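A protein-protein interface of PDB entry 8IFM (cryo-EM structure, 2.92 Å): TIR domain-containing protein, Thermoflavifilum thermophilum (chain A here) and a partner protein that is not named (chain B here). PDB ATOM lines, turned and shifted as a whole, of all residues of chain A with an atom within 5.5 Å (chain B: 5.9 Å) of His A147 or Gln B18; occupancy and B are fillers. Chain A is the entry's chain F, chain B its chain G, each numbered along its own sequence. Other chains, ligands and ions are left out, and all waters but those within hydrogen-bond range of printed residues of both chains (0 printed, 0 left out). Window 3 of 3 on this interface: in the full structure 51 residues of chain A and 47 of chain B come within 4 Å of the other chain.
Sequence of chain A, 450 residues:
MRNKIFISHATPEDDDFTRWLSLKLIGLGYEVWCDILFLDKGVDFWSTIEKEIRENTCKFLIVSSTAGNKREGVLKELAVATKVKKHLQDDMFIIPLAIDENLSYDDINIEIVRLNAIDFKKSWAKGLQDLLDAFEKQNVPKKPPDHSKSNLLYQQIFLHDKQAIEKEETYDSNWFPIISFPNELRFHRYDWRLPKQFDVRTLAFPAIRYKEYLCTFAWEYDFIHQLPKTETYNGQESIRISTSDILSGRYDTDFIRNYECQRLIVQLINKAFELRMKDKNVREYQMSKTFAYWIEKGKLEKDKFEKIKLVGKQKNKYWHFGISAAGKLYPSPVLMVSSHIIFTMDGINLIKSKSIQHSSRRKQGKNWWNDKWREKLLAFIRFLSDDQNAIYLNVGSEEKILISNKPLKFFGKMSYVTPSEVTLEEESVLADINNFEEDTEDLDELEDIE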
ATOM      1  N   LYS A  24     -19.304  21.268  12.521  1.00  0.00           N
ATOM      2  CA  LYS A  24     -19.719  21.606  11.162  1.00  0.00           C
ATOM      3  C   LYS A  24     -18.530  21.596  10.209  1.00  0.00           C
ATOM      4  O   LYS A  24     -18.570  20.948   9.157  1.00  0.00           O
ATOM      5  CB  LYS A  24     -20.418  22.966  11.134  1.00  0.00           C
ATOM      6  CG  LYS A  24     -21.658  23.057  12.004  1.00  0.00           C
ATOM      7  CD  LYS A  24     -22.771  22.175  11.471  1.00  0.00           C
ATOM      8  CE  LYS A  24     -23.707  22.951  10.563  1.00  0.00           C
ATOM      9  NZ  LYS A  24     -24.492  22.047   9.678  1.00  0.00           N
ATOM     10  N   GLY A  27     -17.504  18.442   9.286  1.00  0.00           N
ATOM     11  CA  GLY A  27     -18.499  17.895   8.376  1.00  0.00           C
ATOM     12  C   GLY A  27     -18.236  18.262   6.927  1.00  0.00           C
ATOM     13  O   GLY A  27     -18.292  17.408   6.038  1.00  0.00           O
ATOM     14  N   LEU A  28     -17.939  19.538   6.666  1.00  0.00           N
ATOM     15  CA  LEU A  28     -17.661  19.943   5.290  1.00  0.00           C
ATOM     16  C   LEU A  28     -16.343  19.394   4.755  1.00  0.00           C
ATOM     17  O   LEU A  28     -16.113  19.473   3.544  1.00  0.00           O
ATOM     18  CB  LEU A  28     -17.666  21.468   5.127  1.00  0.00           C
ATOM     19  CG  LEU A  28     -18.930  22.304   5.370  1.00  0.00           C
ATOM     20  CD1 LEU A  28     -20.164  21.613   4.792  1.00  0.00           C
ATOM     21  CD2 LEU A  28     -19.136  22.700   6.816  1.00  0.00           C
ATOM     22  N   PRO A 145     -16.501  16.493   1.533  1.00  0.00           N
ATOM     23  CA  PRO A 145     -17.295  16.509   2.767  1.00  0.00           C
ATOM     24  C   PRO A 145     -17.719  15.102   3.162  1.00  0.00           C
ATOM     25  O   PRO A 145     -18.226  14.337   2.340  1.00  0.00           O
ATOM     26  CB  PRO A 145     -18.505  17.385   2.408  1.00  0.00           C
ATOM     27  CG  PRO A 145     -18.260  17.881   0.996  1.00  0.00           C
ATOM     28  CD  PRO A 145     -17.283  16.945   0.374  1.00  0.00           C
ATOM     29  N   ASP A 146     -17.505  14.767   4.435  1.00  0.00           N
ATOM     30  CA  ASP A 146     -17.882  13.464   4.986  1.00  0.00           C
ATOM     31  C   ASP A 146     -18.442  13.719   6.384  1.00  0.00           C
ATOM     32  O   ASP A 146     -17.690  13.802   7.360  1.00  0.00           O
ATOM     33  CB  ASP A 146     -16.698  12.506   5.010  1.00  0.00           C
ATOM     34  CG  ASP A 146     -17.124  11.052   5.032  1.00  0.00           C
ATOM     35  OD1 ASP A 146     -17.782  10.608   4.068  1.00  0.00           O
ATOM     36  OD2 ASP A 146     -16.800  10.351   6.013  1.00  0.00           O
ATOM     37  N   HIS A 147     -19.767  13.848   6.471  1.00  0.00           N
ATOM     38  CA  HIS A 147     -20.411  14.140   7.747  1.00  0.00           C
ATOM     39  C   HIS A 147     -20.325  12.972   8.719  1.00  0.00           C
ATOM     40  O   HIS A 147     -20.532  13.167   9.924  1.00  0.00           O
ATOM     41  CB  HIS A 147     -21.871  14.529   7.518  1.00  0.00           C
ATOM     42  CG  HIS A 147     -22.088  16.004   7.388  1.00  0.00           C
ATOM     43  ND1 HIS A 147     -22.240  16.834   8.477  1.00  0.00           N
ATOM     44  CD2 HIS A 147     -22.170  16.800   6.295  1.00  0.00           C
ATOM     45  CE1 HIS A 147     -22.411  18.076   8.062  1.00  0.00           C
ATOM     46  NE2 HIS A 147     -22.372  18.082   6.742  1.00  0.00           N
ATOM     47  N   SER A 148     -20.033  11.767   8.225  1.00  0.00           N
ATOM     48  CA  SER A 148     -19.826  10.634   9.118  1.00  0.00           C
ATOM     49  C   SER A 148     -18.650  10.875  10.051  1.00  0.00           C
ATOM     50  O   SER A 148     -18.673  10.432  11.204  1.00  0.00           O
ATOM     51  CB  SER A 148     -19.613   9.355   8.307  1.00  0.00           C
ATOM     52  OG  SER A 148     -18.801   9.600   7.174  1.00  0.00           O
ATOM     53  N   LYS A 149     -17.620  11.581   9.578  1.00  0.00           N
ATOM     54  CA  LYS A 149     -16.514  11.953  10.455  1.00  0.00           C
ATOM     55  C   LYS A 149     -16.987  12.866  11.577  1.00  0.00           C
ATOM     56  O   LYS A 149     -16.572  12.709  12.731  1.00  0.00           O
ATOM     57  CB  LYS A 149     -15.406  12.631   9.649  1.00  0.00           C
ATOM     58  CG  LYS A 149     -15.087  11.954   8.329  1.00  0.00           C
ATOM     59  CD  LYS A 149     -13.655  12.228   7.904  1.00  0.00           C
ATOM     60  CE  LYS A 149     -13.338  11.566   6.574  1.00  0.00           C
ATOM     61  NZ  LYS A 149     -12.905  10.153   6.745  1.00  0.00           N
ATOM     62  N   SER A 150     -17.852  13.832  11.258  1.00  0.00           N
ATOM     63  CA  SER A 150     -18.384  14.719  12.287  1.00  0.00           C
ATOM     64  C   SER A 150     -19.235  13.954  13.291  1.00  0.00           C
ATOM     65  O   SER A 150     -19.153  14.198  14.499  1.00  0.00           O
ATOM     66  CB  SER A 150     -19.195  15.842  11.643  1.00  0.00           C
ATOM     67  OG  SER A 150     -19.347  16.933  12.534  1.00  0.00           O
ATOM     68  N   ASN A 151     -20.060  13.021  12.809  1.00  0.00           N
ATOM     69  CA  ASN A 151     -20.862  12.204  13.717  1.00  0.00           C
ATOM     70  C   ASN A 151     -19.976  11.361  14.625  1.00  0.00           C
ATOM     71  O   ASN A 151     -20.220  11.265  15.837  1.00  0.00           O
ATOM     72  CB  ASN A 151     -21.813  11.314  12.918  1.00  0.00           C
ATOM     73  CG  ASN A 151     -22.987  10.826  13.741  1.00  0.00           C
ATOM     74  OD1 ASN A 151     -23.136  11.190  14.907  1.00  0.00           O
ATOM     75  ND2 ASN A 151     -23.827   9.996  13.136  1.00  0.00           N
ATOM     76  N   LEU A 152     -18.934  10.749  14.059  1.00  0.00           N
ATOM     77  CA  LEU A 152     -18.007   9.963  14.864  1.00  0.00           C
ATOM     78  C   LEU A 152     -17.337  10.830  15.920  1.00  0.00           C
ATOM     79  O   LEU A 152     -17.287  10.459  17.094  1.00  0.00           O
ATOM     80  CB  LEU A 152     -16.963   9.303  13.964  1.00  0.00           C
ATOM     81  CG  LEU A 152     -16.756   7.796  14.134  1.00  0.00           C
ATOM     82  CD1 LEU A 152     -18.078   7.054  14.023  1.00  0.00           C
ATOM     83  CD2 LEU A 152     -15.758   7.274  13.114  1.00  0.00           C
ATOM     84  N   ILE B  12     -32.614   7.916  14.985  1.00  0.00           N
ATOM     85  CA  ILE B  12     -33.425   8.629  14.006  1.00  0.00           C
ATOM     86  C   ILE B  12     -32.500   9.259  12.976  1.00  0.00           C
ATOM     87  O   ILE B  12     -31.499   9.895  13.330  1.00  0.00           O
ATOM     88  CB  ILE B  12     -34.310   9.686  14.688  1.00  0.00           C
ATOM     89  CG1 ILE B  12     -33.518  10.475  15.726  1.00  0.00           C
ATOM     90  CG2 ILE B  12     -35.496   9.029  15.364  1.00  0.00           C
ATOM     91  CD1 ILE B  12     -34.310  11.569  16.387  1.00  0.00           C
ATOM     92  N   LEU B  13     -32.818   9.065  11.699  1.00  0.00           N
ATOM     93  CA  LEU B  13     -31.972   9.564  10.627  1.00  0.00           C
ATOM     94  C   LEU B  13     -32.061  11.085  10.522  1.00  0.00           C
ATOM     95  O   LEU B  13     -33.014  11.716  10.984  1.00  0.00           O
ATOM     96  CB  LEU B  13     -32.361   8.925   9.295  1.00  0.00           C
ATOM     97  CG  LEU B  13     -32.059   7.432   9.158  1.00  0.00           C
ATOM     98  CD1 LEU B  13     -32.184   6.982   7.714  1.00  0.00           C
ATOM     99  CD2 LEU B  13     -30.674   7.126   9.688  1.00  0.00           C
ATOM    100  N   PHE B  14     -31.041  11.669   9.898  1.00  0.00           N
ATOM    101  CA  PHE B  14     -30.968  13.107   9.680  1.00  0.00           C
ATOM    102  C   PHE B  14     -30.395  13.347   8.288  1.00  0.00           C
ATOM    103  O   PHE B  14     -30.320  12.434   7.459  1.00  0.00           O
ATOM    104  CB  PHE B  14     -30.130  13.786  10.770  1.00  0.00           C
ATOM    105  CG  PHE B  14     -30.796  13.819  12.108  1.00  0.00           C
ATOM    106  CD1 PHE B  14     -31.692  14.823  12.425  1.00  0.00           C
ATOM    107  CD2 PHE B  14     -30.525  12.848  13.052  1.00  0.00           C
ATOM    108  CE1 PHE B  14     -32.305  14.855  13.659  1.00  0.00           C
ATOM    109  CE2 PHE B  14     -31.135  12.876  14.286  1.00  0.00           C
ATOM    110  CZ  PHE B  14     -32.026  13.878  14.589  1.00  0.00           C
ATOM    111  N   ALA B  15     -29.990  14.587   8.030  1.00  0.00           N
ATOM    112  CA  ALA B  15     -29.413  14.931   6.738  1.00  0.00           C
ATOM    113  C   ALA B  15     -28.107  14.178   6.517  1.00  0.00           C
ATOM    114  O   ALA B  15     -27.387  13.844   7.462  1.00  0.00           O
ATOM    115  CB  ALA B  15     -29.170  16.437   6.644  1.00  0.00           C
ATOM    116  N   HIS B  16     -27.818  13.898   5.246  1.00  0.00           N
ATOM    117  CA  HIS B  16     -26.598  13.227   4.805  1.00  0.00           C
ATOM    118  C   HIS B  16     -26.484  11.802   5.336  1.00  0.00           C
ATOM    119  O   HIS B  16     -25.391  11.228   5.339  1.00  0.00           O
ATOM    120  CB  HIS B  16     -25.347  14.029   5.187  1.00  0.00           C
ATOM    121  CG  HIS B  16     -25.518  15.511   5.060  1.00  0.00           C
ATOM    122  ND1 HIS B  16     -25.567  16.154   3.843  1.00  0.00           N
ATOM    123  CD2 HIS B  16     -25.648  16.477   6.001  1.00  0.00           C
ATOM    124  CE1 HIS B  16     -25.721  17.452   4.038  1.00  0.00           C
ATOM    125  NE2 HIS B  16     -25.773  17.674   5.339  1.00  0.00           N
ATOM    126  N   GLY B  17     -27.589  11.214   5.789  1.00  0.00           N
ATOM    127  CA  GLY B  17     -27.569   9.843   6.257  1.00  0.00           C
ATOM    128  C   GLY B  17     -26.945   9.631   7.615  1.00  0.00           C
ATOM    129  O   GLY B  17     -26.545   8.507   7.930  1.00  0.00           O
ATOM    130  N   GLN B  18     -26.850  10.674   8.435  1.00  0.00           N
ATOM    131  CA  GLN B  18     -26.221  10.590   9.747  1.00  0.00           C
ATOM    132  C   GLN B  18     -27.288  10.333  10.803  1.00  0.00           C
ATOM    133  O   GLN B  18     -28.220  11.130  10.957  1.00  0.00           O
ATOM    134  CB  GLN B  18     -25.447  11.868  10.062  1.00  0.00           C
ATOM    135  CG  GLN B  18     -24.245  12.088   9.166  1.00  0.00           C
ATOM    136  CD  GLN B  18     -23.571  10.788   8.775  1.00  0.00           C
ATOM    137  OE1 GLN B  18     -23.026  10.078   9.620  1.00  0.00           O
ATOM    138  NE2 GLN B  18     -23.608  10.468   7.487  1.00  0.00           N
ATOM    139  N   LYS B  19     -27.143   9.231  11.531  1.00  0.00           N
ATOM    140  CA  LYS B  19     -28.110   8.819  12.537  1.00  0.00           C
ATOM    141  C   LYS B  19     -27.624   9.223  13.924  1.00  0.00           C
ATOM    142  O   LYS B  19     -26.472   8.963  14.287  1.00  0.00           O
ATOM    143  CB  LYS B  19     -28.349   7.309  12.465  1.00  0.00           C
ATOM    144  CG  LYS B  19     -27.084   6.465  12.558  1.00  0.00           C
ATOM    145  CD  LYS B  19     -27.391   4.976  12.665  1.00  0.00           C
ATOM    146  CE  LYS B  19     -28.520   4.548  11.738  1.00  0.00           C
ATOM    147  NZ  LYS B  19     -28.284   4.959  10.323  1.00  0.00           N
ATOM    148  N   CYS B  20     -28.499   9.875  14.684  1.00  0.00           N
ATOM    149  CA  CYS B  20     -28.219  10.247  16.062  1.00  0.00           C
ATOM    150  C   CYS B  20     -29.460   9.974  16.898  1.00  0.00           C
ATOM    151  O   CYS B  20     -30.582  10.012  16.393  1.00  0.00           O
ATOM    152  CB  CYS B  20     -27.808  11.720  16.175  1.00  0.00           C
ATOM    153  SG  CYS B  20     -27.943  12.415  17.837  1.00  0.00           S
ATOM    154  N   LEU B  29     -26.337  19.052  14.431  1.00  0.00           N
ATOM    155  CA  LEU B  29     -25.134  18.503  13.817  1.00  0.00           C
ATOM    156  C   LEU B  29     -25.279  18.368  12.306  1.00  0.00           C
ATOM    157  O   LEU B  29     -24.361  18.725  11.558  1.00  0.00           O
ATOM    158  CB  LEU B  29     -24.811  17.147  14.445  1.00  0.00           C
ATOM    159  CG  LEU B  29     -23.687  17.093  15.478  1.00  0.00           C
ATOM    160  CD1 LEU B  29     -22.393  17.555  14.844  1.00  0.00           C
ATOM    161  CD2 LEU B  29     -24.021  17.938  16.698  1.00  0.00           C
ATOM    162  N   PHE B  30     -26.409  17.856  11.839  1.00  0.00           N
ATOM    163  CA  PHE B  30     -26.518  17.498  10.427  1.00  0.00           C
ATOM    164  C   PHE B  30     -27.666  18.188   9.707  1.00  0.00           C
ATOM    165  O   PHE B  30     -27.500  18.593   8.554  1.00  0.00           O
ATOM    166  CB  PHE B  30     -26.657  15.976  10.301  1.00  0.00           C
ATOM    167  CG  PHE B  30     -25.873  15.214  11.327  1.00  0.00           C
ATOM    168  CD1 PHE B  30     -24.489  15.214  11.300  1.00  0.00           C
ATOM    169  CD2 PHE B  30     -26.517  14.507  12.325  1.00  0.00           C
ATOM    170  CE1 PHE B  30     -23.765  14.520  12.246  1.00  0.00           C
ATOM    171  CE2 PHE B  30     -25.798  13.812  13.273  1.00  0.00           C
ATOM    172  CZ  PHE B  30     -24.421  13.817  13.233  1.00  0.00           C
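Of the printed residues of chain B, Lys A24 touches Leu B29.
Of chain B, only His B16 (3.5 Å), Gln B18 (3.8 Å) and Phe B30 (3.96 Å) come within 4 Å of His A147.
Of the printed residues of chain B, Asn A151 touches Gln B18 (3.6 Å), Lys B19 (3.1 Å) and Phe B30 (3.4 Å).
Leu B13 touches none of the printed residues of chain A.
Of the printed residues of chain A, Lys B19 touches Asn A151.
The nearest residue of chain B that does not touch His A147 is Leu B29 (4.1 Å).
The nearest printed residue of chain B that does not touch Ser A150 is Phe B30 (4.7 Å).
Among the printed residues, merely in contact across the chains: Lys A24 with Leu B29, His A147 with His B16, His A147 with Gln B18, His A147 with Phe B30, Ser A148 with Gln B18, Ser A150 with Leu B29, Asn A151 with Gln B18 and Asn A151 with Phe B30.
The backbone carbonyl oxygen (O) of His B16 lies within hydrogen-bond range of the side-chain amide nitrogen (NE2) of Gln B18 (2.9 Å).
The side-chain hydroxyl of Ser A148 sits at hydrogen-bond distance from the side-chain carboxylate of Asp A146, 2.4 Å away.
Hydrophobic or aromatic side chains of chain A that line the printed part of chain B: His A147.
The side-chain amide nitrogen (ND2) of Asn A151 is in hydrogen-bond range of the backbone carbonyl oxygen (O) of Lys B19 (3.1 Å).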
